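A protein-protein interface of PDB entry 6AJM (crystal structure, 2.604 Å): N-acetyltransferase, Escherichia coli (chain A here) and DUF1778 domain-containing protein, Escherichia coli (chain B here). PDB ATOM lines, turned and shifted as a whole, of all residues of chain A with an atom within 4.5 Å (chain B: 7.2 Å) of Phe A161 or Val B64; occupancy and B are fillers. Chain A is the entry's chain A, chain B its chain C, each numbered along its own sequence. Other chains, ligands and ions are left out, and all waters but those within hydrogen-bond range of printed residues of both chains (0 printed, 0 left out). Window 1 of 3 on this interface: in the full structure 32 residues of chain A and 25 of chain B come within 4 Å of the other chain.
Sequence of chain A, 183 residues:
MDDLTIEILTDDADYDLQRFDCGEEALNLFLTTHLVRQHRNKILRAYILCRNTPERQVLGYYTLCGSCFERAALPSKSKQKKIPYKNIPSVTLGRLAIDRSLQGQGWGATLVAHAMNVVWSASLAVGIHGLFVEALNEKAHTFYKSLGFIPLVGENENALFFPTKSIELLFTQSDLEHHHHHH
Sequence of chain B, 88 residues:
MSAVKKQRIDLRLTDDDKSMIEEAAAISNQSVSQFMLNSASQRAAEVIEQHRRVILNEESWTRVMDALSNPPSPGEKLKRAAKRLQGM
The backbone NH (N) of Ile A150 lies within hydrogen-bond range of the backbone carbonyl oxygen (O) of Phe A161 (2.9 Å). O of Met B65 lies within hydrogen-bond range of OG of Ser B69 (3.4 Å). NE of Arg B63 lies within salt-bridge range of OE2 of Glu B59, at 3.999 Å.
Among the printed residues, merely in contact across the chains: His A129 with Leu B68 (3.4 Å), Pro A163 with Pro B72 (3.5 Å), Leu A152 with Ser B60 (3.6 Å), Phe A69 with Leu B56 (3.7 Å), Phe A69 with Val B64 (3.7 Å), Pro A163 with Ala B67 (3.8 Å), Ile A150 with Arg B63 (3.9 Å), Phe A69 with Met B65 (3.9 Å), Phe A69 with Trp B61 (3.9 Å), Phe A161 with Val B64 (3.9 Å) and Ile A150 with Pro B72 (3.9 Å).
Printed residues of chain B within 4 Å of His A129: Leu B68 (3.4 Å). Of chain B, only Val B64 comes within 4 Å of Phe A161. Printed residues of chain A within 4 Å of Trp B61: Phe A69 (3.9 Å). Of the printed residues of chain A, Val B64 touches Phe A69 (3.7 Å) and Phe A161 (3.9 Å). The nearest residue of chain A that does not touch Val B64 is Leu A152 (4.2 Å). The nearest printed residue of chain B that does not touch Phe A69 is Leu B68 (4.7 Å).
Hydrophobic or aromatic side chains of chain B within 4 Å of the printed part of chain A: Leu B56, Trp B61, Val B64, Met B65, Leu B68 and Pro B72. Among the printed residues, no Asp or Glu carboxylate lies within 4 Å of a Lys or Arg side-chain nitrogen of the other chain.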
ATOM      1  N   PHE A  69      32.158   7.789 -11.594  1.00  0.00           N
ATOM      2  CA  PHE A  69      31.279   8.561 -12.468  1.00  0.00           C
ATOM      3  C   PHE A  69      30.233   9.359 -11.688  1.00  0.00           C
ATOM      4  O   PHE A  69      29.963   9.103 -10.515  1.00  0.00           O
ATOM      5  CB  PHE A  69      30.604   7.670 -13.531  1.00  0.00           C
ATOM      6  CG  PHE A  69      29.858   6.482 -12.978  1.00  0.00           C
ATOM      7  CD1 PHE A  69      28.479   6.418 -13.095  1.00  0.00           C
ATOM      8  CD2 PHE A  69      30.521   5.428 -12.383  1.00  0.00           C
ATOM      9  CE1 PHE A  69      27.774   5.342 -12.608  1.00  0.00           C
ATOM     10  CE2 PHE A  69      29.817   4.339 -11.897  1.00  0.00           C
ATOM     11  CZ  PHE A  69      28.440   4.298 -12.016  1.00  0.00           C
ATOM     12  N   HIS A 129      31.040  -0.829  -9.504  1.00  0.00           N
ATOM     13  CA  HIS A 129      29.742  -0.998 -10.145  1.00  0.00           C
ATOM     14  C   HIS A 129      29.842  -1.506 -11.578  1.00  0.00           C
ATOM     15  O   HIS A 129      28.900  -2.144 -12.064  1.00  0.00           O
ATOM     16  CB  HIS A 129      28.975   0.315 -10.119  1.00  0.00           C
ATOM     17  CG  HIS A 129      28.313   0.583  -8.813  1.00  0.00           C
ATOM     18  ND1 HIS A 129      28.940   1.256  -7.788  1.00  0.00           N
ATOM     19  CD2 HIS A 129      27.081   0.259  -8.359  1.00  0.00           C
ATOM     20  CE1 HIS A 129      28.112   1.355  -6.763  1.00  0.00           C
ATOM     21  NE2 HIS A 129      26.977   0.760  -7.085  1.00  0.00           N
ATOM     22  N   GLY A 130      30.942  -1.229 -12.269  1.00  0.00           N
ATOM     23  CA  GLY A 130      31.044  -1.616 -13.662  1.00  0.00           C
ATOM     24  C   GLY A 130      32.355  -1.150 -14.256  1.00  0.00           C
ATOM     25  O   GLY A 130      33.216  -0.594 -13.563  1.00  0.00           O
ATOM     26  N   LEU A 131      32.459  -1.345 -15.575  1.00  0.00           N
ATOM     27  CA  LEU A 131      33.701  -1.250 -16.331  1.00  0.00           C
ATOM     28  C   LEU A 131      33.478  -0.396 -17.568  1.00  0.00           C
ATOM     29  O   LEU A 131      32.814  -0.840 -18.510  1.00  0.00           O
ATOM     30  CB  LEU A 131      34.162  -2.650 -16.745  1.00  0.00           C
ATOM     31  CG  LEU A 131      35.615  -3.019 -17.070  1.00  0.00           C
ATOM     32  CD1 LEU A 131      35.649  -3.955 -18.246  1.00  0.00           C
ATOM     33  CD2 LEU A 131      36.531  -1.839 -17.303  1.00  0.00           C
ATOM     34  N   PHE A 132      34.052   0.806 -17.579  1.00  0.00           N
ATOM     35  CA  PHE A 132      34.117   1.629 -18.788  1.00  0.00           C
ATOM     36  C   PHE A 132      35.310   1.227 -19.657  1.00  0.00           C
ATOM     37  O   PHE A 132      36.339   0.779 -19.153  1.00  0.00           O
ATOM     38  CB  PHE A 132      34.260   3.116 -18.430  1.00  0.00           C
ATOM     39  CG  PHE A 132      33.135   3.678 -17.599  1.00  0.00           C
ATOM     40  CD1 PHE A 132      32.052   4.309 -18.204  1.00  0.00           C
ATOM     41  CD2 PHE A 132      33.177   3.619 -16.202  1.00  0.00           C
ATOM     42  CE1 PHE A 132      31.015   4.851 -17.435  1.00  0.00           C
ATOM     43  CE2 PHE A 132      32.141   4.152 -15.426  1.00  0.00           C
ATOM     44  CZ  PHE A 132      31.065   4.767 -16.043  1.00  0.00           C
ATOM     45  N   GLY A 148      29.218  -6.791 -25.630  1.00  0.00           N
ATOM     46  CA  GLY A 148      28.201  -6.438 -24.664  1.00  0.00           C
ATOM     47  C   GLY A 148      28.298  -5.025 -24.145  1.00  0.00           C
ATOM     48  O   GLY A 148      27.352  -4.572 -23.491  1.00  0.00           O
ATOM     49  N   PHE A 149      29.381  -4.295 -24.421  1.00  0.00           N
ATOM     50  CA  PHE A 149      29.517  -2.929 -23.921  1.00  0.00           C
ATOM     51  C   PHE A 149      28.449  -2.015 -24.513  1.00  0.00           C
ATOM     52  O   PHE A 149      28.215  -2.012 -25.730  1.00  0.00           O
ATOM     53  CB  PHE A 149      30.910  -2.384 -24.239  1.00  0.00           C
ATOM     54  CG  PHE A 149      31.984  -2.917 -23.339  1.00  0.00           C
ATOM     55  CD1 PHE A 149      32.437  -4.222 -23.461  1.00  0.00           C
ATOM     56  CD2 PHE A 149      32.545  -2.110 -22.362  1.00  0.00           C
ATOM     57  CE1 PHE A 149      33.435  -4.709 -22.605  1.00  0.00           C
ATOM     58  CE2 PHE A 149      33.535  -2.590 -21.508  1.00  0.00           C
ATOM     59  CZ  PHE A 149      33.985  -3.884 -21.631  1.00  0.00           C
ATOM     60  N   ILE A 150      27.799  -1.240 -23.648  1.00  0.00           N
ATOM     61  CA  ILE A 150      26.746  -0.327 -24.087  1.00  0.00           C
ATOM     62  C   ILE A 150      27.355   1.020 -24.458  1.00  0.00           C
ATOM     63  O   ILE A 150      28.030   1.641 -23.622  1.00  0.00           O
ATOM     64  CB  ILE A 150      25.661  -0.151 -23.013  1.00  0.00           C
ATOM     65  CG1 ILE A 150      24.874  -1.453 -22.813  1.00  0.00           C
ATOM     66  CG2 ILE A 150      24.711   0.998 -23.389  1.00  0.00           C
ATOM     67  CD1 ILE A 150      25.285  -2.242 -21.582  1.00  0.00           C
ATOM     68  N   LEU A 152      27.747   5.011 -25.046  1.00  0.00           N
ATOM     69  CA  LEU A 152      27.269   6.256 -24.473  1.00  0.00           C
ATOM     70  C   LEU A 152      27.258   7.311 -25.573  1.00  0.00           C
ATOM     71  O   LEU A 152      28.042   7.243 -26.523  1.00  0.00           O
ATOM     72  CB  LEU A 152      28.165   6.680 -23.308  1.00  0.00           C
ATOM     73  CG  LEU A 152      27.934   6.018 -21.934  1.00  0.00           C
ATOM     74  CD1 LEU A 152      27.000   4.805 -21.979  1.00  0.00           C
ATOM     75  CD2 LEU A 152      29.252   5.656 -21.248  1.00  0.00           C
ATOM     76  N   LEU A 160      32.240   3.274 -23.537  1.00  0.00           N
ATOM     77  CA  LEU A 160      31.199   2.274 -23.406  1.00  0.00           C
ATOM     78  C   LEU A 160      31.305   1.672 -22.020  1.00  0.00           C
ATOM     79  O   LEU A 160      32.327   1.820 -21.342  1.00  0.00           O
ATOM     80  CB  LEU A 160      31.311   1.186 -24.473  1.00  0.00           C
ATOM     81  CG  LEU A 160      31.316   1.655 -25.923  1.00  0.00           C
ATOM     82  CD1 LEU A 160      32.710   2.118 -26.367  1.00  0.00           C
ATOM     83  CD2 LEU A 160      30.805   0.540 -26.817  1.00  0.00           C
ATOM     84  N   PHE A 161      30.246   0.972 -21.607  1.00  0.00           N
ATOM     85  CA  PHE A 161      30.117   0.526 -20.224  1.00  0.00           C
ATOM     86  C   PHE A 161      29.617  -0.909 -20.152  1.00  0.00           C
ATOM     87  O   PHE A 161      28.772  -1.317 -20.950  1.00  0.00           O
ATOM     88  CB  PHE A 161      29.152   1.439 -19.448  1.00  0.00           C
ATOM     89  CG  PHE A 161      28.918   1.010 -18.019  1.00  0.00           C
ATOM     90  CD1 PHE A 161      29.845   1.306 -17.025  1.00  0.00           C
ATOM     91  CD2 PHE A 161      27.768   0.329 -17.669  1.00  0.00           C
ATOM     92  CE1 PHE A 161      29.633   0.921 -15.713  1.00  0.00           C
ATOM     93  CE2 PHE A 161      27.553  -0.058 -16.354  1.00  0.00           C
ATOM     94  CZ  PHE A 161      28.486   0.241 -15.378  1.00  0.00           C
ATOM     95  N   PHE A 162      30.122  -1.661 -19.161  1.00  0.00           N
ATOM     96  CA  PHE A 162      29.654  -3.015 -18.871  1.00  0.00           C
ATOM     97  C   PHE A 162      29.443  -3.198 -17.369  1.00  0.00           C
ATOM     98  O   PHE A 162      30.391  -3.032 -16.591  1.00  0.00           O
ATOM     99  CB  PHE A 162      30.659  -4.044 -19.388  1.00  0.00           C
ATOM    100  CG  PHE A 162      30.068  -5.395 -19.659  1.00  0.00           C
ATOM    101  CD1 PHE A 162      29.034  -5.546 -20.570  1.00  0.00           C
ATOM    102  CD2 PHE A 162      30.565  -6.524 -19.025  1.00  0.00           C
ATOM    103  CE1 PHE A 162      28.502  -6.811 -20.846  1.00  0.00           C
ATOM    104  CE2 PHE A 162      30.036  -7.778 -19.289  1.00  0.00           C
ATOM    105  CZ  PHE A 162      29.004  -7.921 -20.203  1.00  0.00           C
ATOM    106  N   PRO A 163      28.234  -3.542 -16.917  1.00  0.00           N
ATOM    107  CA  PRO A 163      28.013  -3.692 -15.474  1.00  0.00           C
ATOM    108  C   PRO A 163      28.805  -4.847 -14.888  1.00  0.00           C
ATOM    109  O   PRO A 163      29.019  -5.883 -15.524  1.00  0.00           O
ATOM    110  CB  PRO A 163      26.501  -3.941 -15.358  1.00  0.00           C
ATOM    111  CG  PRO A 163      26.079  -4.457 -16.692  1.00  0.00           C
ATOM    112  CD  PRO A 163      26.998  -3.771 -17.687  1.00  0.00           C
ATOM    113  N   LEU B  56      28.752  12.167 -16.835  1.00  0.00           N
ATOM    114  CA  LEU B  56      27.805  11.567 -17.762  1.00  0.00           C
ATOM    115  C   LEU B  56      26.658  12.531 -17.976  1.00  0.00           C
ATOM    116  O   LEU B  56      26.079  13.031 -17.008  1.00  0.00           O
ATOM    117  CB  LEU B  56      27.282  10.231 -17.235  1.00  0.00           C
ATOM    118  CG  LEU B  56      28.344   9.163 -16.906  1.00  0.00           C
ATOM    119  CD1 LEU B  56      27.711   7.852 -16.414  1.00  0.00           C
ATOM    120  CD2 LEU B  56      29.213   8.890 -18.084  1.00  0.00           C
ATOM    121  N   GLU B  59      21.573  11.351 -20.949  1.00  0.00           N
ATOM    122  CA  GLU B  59      21.283  10.080 -21.613  1.00  0.00           C
ATOM    123  C   GLU B  59      22.333   8.998 -21.332  1.00  0.00           C
ATOM    124  O   GLU B  59      21.984   7.817 -21.183  1.00  0.00           O
ATOM    125  CB  GLU B  59      21.143  10.316 -23.118  1.00  0.00           C
ATOM    126  CG  GLU B  59      20.843   9.071 -23.923  1.00  0.00           C
ATOM    127  CD  GLU B  59      19.467   8.499 -23.632  1.00  0.00           C
ATOM    128  OE1 GLU B  59      18.655   9.176 -22.958  1.00  0.00           O
ATOM    129  OE2 GLU B  59      19.194   7.366 -24.085  1.00  0.00           O
ATOM    130  N   SER B  60      23.615   9.356 -21.261  1.00  0.00           N
ATOM    131  CA  SER B  60      24.604   8.360 -20.864  1.00  0.00           C
ATOM    132  C   SER B  60      24.320   7.862 -19.456  1.00  0.00           C
ATOM    133  O   SER B  60      24.418   6.658 -19.183  1.00  0.00           O
ATOM    134  CB  SER B  60      26.015   8.939 -20.943  1.00  0.00           C
ATOM    135  OG  SER B  60      26.097   9.970 -21.901  1.00  0.00           O
ATOM    136  N   TRP B  61      23.975   8.786 -18.552  1.00  0.00           N
ATOM    137  CA  TRP B  61      23.584   8.413 -17.198  1.00  0.00           C
ATOM    138  C   TRP B  61      22.403   7.464 -17.224  1.00  0.00           C
ATOM    139  O   TRP B  61      22.397   6.448 -16.523  1.00  0.00           O
ATOM    140  CB  TRP B  61      23.236   9.661 -16.383  1.00  0.00           C
ATOM    141  CG  TRP B  61      22.734   9.373 -14.978  1.00  0.00           C
ATOM    142  CD1 TRP B  61      21.432   9.335 -14.556  1.00  0.00           C
ATOM    143  CD2 TRP B  61      23.537   9.092 -13.822  1.00  0.00           C
ATOM    144  NE1 TRP B  61      21.379   9.049 -13.212  1.00  0.00           N
ATOM    145  CE2 TRP B  61      22.656   8.896 -12.738  1.00  0.00           C
ATOM    146  CE3 TRP B  61      24.913   8.993 -13.601  1.00  0.00           C
ATOM    147  CZ2 TRP B  61      23.112   8.609 -11.453  1.00  0.00           C
ATOM    148  CZ3 TRP B  61      25.359   8.701 -12.349  1.00  0.00           C
ATOM    149  CH2 TRP B  61      24.462   8.519 -11.279  1.00  0.00           C
ATOM    150  N   THR B  62      21.377   7.796 -18.007  1.00  0.00           N
ATOM    151  CA  THR B  62      20.239   6.892 -18.134  1.00  0.00           C
ATOM    152  C   THR B  62      20.689   5.483 -18.523  1.00  0.00           C
ATOM    153  O   THR B  62      20.234   4.486 -17.949  1.00  0.00           O
ATOM    154  CB  THR B  62      19.238   7.435 -19.165  1.00  0.00           C
ATOM    155  OG1 THR B  62      18.828   8.765 -18.808  1.00  0.00           O
ATOM    156  CG2 THR B  62      18.019   6.540 -19.225  1.00  0.00           C
ATOM    157  N   ARG B  63      21.581   5.379 -19.506  1.00  0.00           N
ATOM    158  CA  ARG B  63      21.923   4.044 -19.991  1.00  0.00           C
ATOM    159  C   ARG B  63      22.788   3.288 -18.993  1.00  0.00           C
ATOM    160  O   ARG B  63      22.594   2.081 -18.798  1.00  0.00           O
ATOM    161  CB  ARG B  63      22.585   4.125 -21.361  1.00  0.00           C
ATOM    162  CG  ARG B  63      21.547   4.165 -22.473  1.00  0.00           C
ATOM    163  CD  ARG B  63      22.126   3.890 -23.844  1.00  0.00           C
ATOM    164  NE  ARG B  63      22.464   5.114 -24.563  1.00  0.00           N
ATOM    165  CZ  ARG B  63      22.682   5.165 -25.874  1.00  0.00           C
ATOM    166  NH1 ARG B  63      22.590   4.064 -26.607  1.00  0.00           N
ATOM    167  NH2 ARG B  63      22.985   6.315 -26.452  1.00  0.00           N
ATOM    168  N   VAL B  64      23.690   3.977 -18.298  1.00  0.00           N
ATOM    169  CA  VAL B  64      24.439   3.313 -17.235  1.00  0.00           C
ATOM    170  C   VAL B  64      23.502   2.820 -16.141  1.00  0.00           C
ATOM    171  O   VAL B  64      23.644   1.693 -15.640  1.00  0.00           O
ATOM    172  CB  VAL B  64      25.511   4.249 -16.663  1.00  0.00           C
ATOM    173  CG1 VAL B  64      26.226   3.550 -15.501  1.00  0.00           C
ATOM    174  CG2 VAL B  64      26.481   4.679 -17.771  1.00  0.00           C
ATOM    175  N   MET B  65      22.538   3.655 -15.742  1.00  0.00           N
ATOM    176  CA  MET B  65      21.607   3.253 -14.693  1.00  0.00           C
ATOM    177  C   MET B  65      20.834   2.012 -15.110  1.00  0.00           C
ATOM    178  O   MET B  65      20.850   0.999 -14.406  1.00  0.00           O
ATOM    179  CB  MET B  65      20.644   4.395 -14.360  1.00  0.00           C
ATOM    180  CG  MET B  65      21.247   5.473 -13.499  1.00  0.00           C
ATOM    181  SD  MET B  65      22.174   4.753 -12.122  1.00  0.00           S
ATOM    182  CE  MET B  65      23.848   5.140 -12.640  1.00  0.00           C
ATOM    183  N   ASP B  66      20.167   2.069 -16.272  1.00  0.00           N
ATOM    184  CA  ASP B  66      19.405   0.915 -16.742  1.00  0.00           C
ATOM    185  C   ASP B  66      20.279  -0.327 -16.861  1.00  0.00           C
ATOM    186  O   ASP B  66      19.808  -1.447 -16.618  1.00  0.00           O
ATOM    187  CB  ASP B  66      18.742   1.221 -18.085  1.00  0.00           C
ATOM    188  CG  ASP B  66      17.523   2.108 -17.943  1.00  0.00           C
ATOM    189  OD1 ASP B  66      17.267   2.610 -16.827  1.00  0.00           O
ATOM    190  OD2 ASP B  66      16.818   2.293 -18.957  1.00  0.00           O
ATOM    191  N   ALA B  67      21.553  -0.154 -17.232  1.00  0.00           N
ATOM    192  CA  ALA B  67      22.476  -1.281 -17.244  1.00  0.00           C
ATOM    193  C   ALA B  67      22.628  -1.883 -15.852  1.00  0.00           C
ATOM    194  O   ALA B  67      22.628  -3.106 -15.693  1.00  0.00           O
ATOM    195  CB  ALA B  67      23.827  -0.833 -17.793  1.00  0.00           C
ATOM    196  N   LEU B  68      22.742  -1.040 -14.820  1.00  0.00           N
ATOM    197  CA  LEU B  68      22.872  -1.584 -13.468  1.00  0.00           C
ATOM    198  C   LEU B  68      21.562  -2.217 -12.985  1.00  0.00           C
ATOM    199  O   LEU B  68      21.572  -3.282 -12.351  1.00  0.00           O
ATOM    200  CB  LEU B  68      23.333  -0.494 -12.508  1.00  0.00           C
ATOM    201  CG  LEU B  68      24.664   0.176 -12.806  1.00  0.00           C
ATOM    202  CD1 LEU B  68      24.697   1.478 -12.025  1.00  0.00           C
ATOM    203  CD2 LEU B  68      25.853  -0.730 -12.445  1.00  0.00           C
ATOM    204  N   SER B  69      20.426  -1.590 -13.300  1.00  0.00           N
ATOM    205  CA  SER B  69      19.124  -2.111 -12.879  1.00  0.00           C
ATOM    206  C   SER B  69      18.870  -3.496 -13.462  1.00  0.00           C
ATOM    207  O   SER B  69      18.611  -4.460 -12.729  1.00  0.00           O
ATOM    208  CB  SER B  69      18.000  -1.150 -13.292  1.00  0.00           C
ATOM    209  OG  SER B  69      18.113   0.115 -12.655  1.00  0.00           O
ATOM    210  N   ASN B  70      18.915  -3.610 -14.789  1.00  0.00           N
ATOM    211  CA  ASN B  70      18.702  -4.880 -15.476  1.00  0.00           C
ATOM    212  C   ASN B  70      19.921  -5.155 -16.342  1.00  0.00           C
ATOM    213  O   ASN B  70      19.965  -4.765 -17.521  1.00  0.00           O
ATOM    214  CB  ASN B  70      17.416  -4.865 -16.294  1.00  0.00           C
ATOM    215  CG  ASN B  70      16.435  -5.905 -15.810  1.00  0.00           C
ATOM    216  OD1 ASN B  70      15.731  -5.697 -14.818  1.00  0.00           O
ATOM    217  ND2 ASN B  70      16.399  -7.047 -16.490  1.00  0.00           N
ATOM    218  N   PRO B  72      22.776  -6.687 -18.762  1.00  0.00           N
ATOM    219  CA  PRO B  72      22.599  -7.498 -19.967  1.00  0.00           C
ATOM    220  C   PRO B  72      23.295  -8.850 -19.872  1.00  0.00           C
ATOM    221  O   PRO B  72      24.299  -9.020 -19.178  1.00  0.00           O
ATOM    222  CB  PRO B  72      23.237  -6.630 -21.058  1.00  0.00           C
ATOM    223  CG  PRO B  72      24.289  -5.854 -20.335  1.00  0.00           C
ATOM    224  CD  PRO B  72      23.741  -5.594 -18.965  1.00  0.00           C
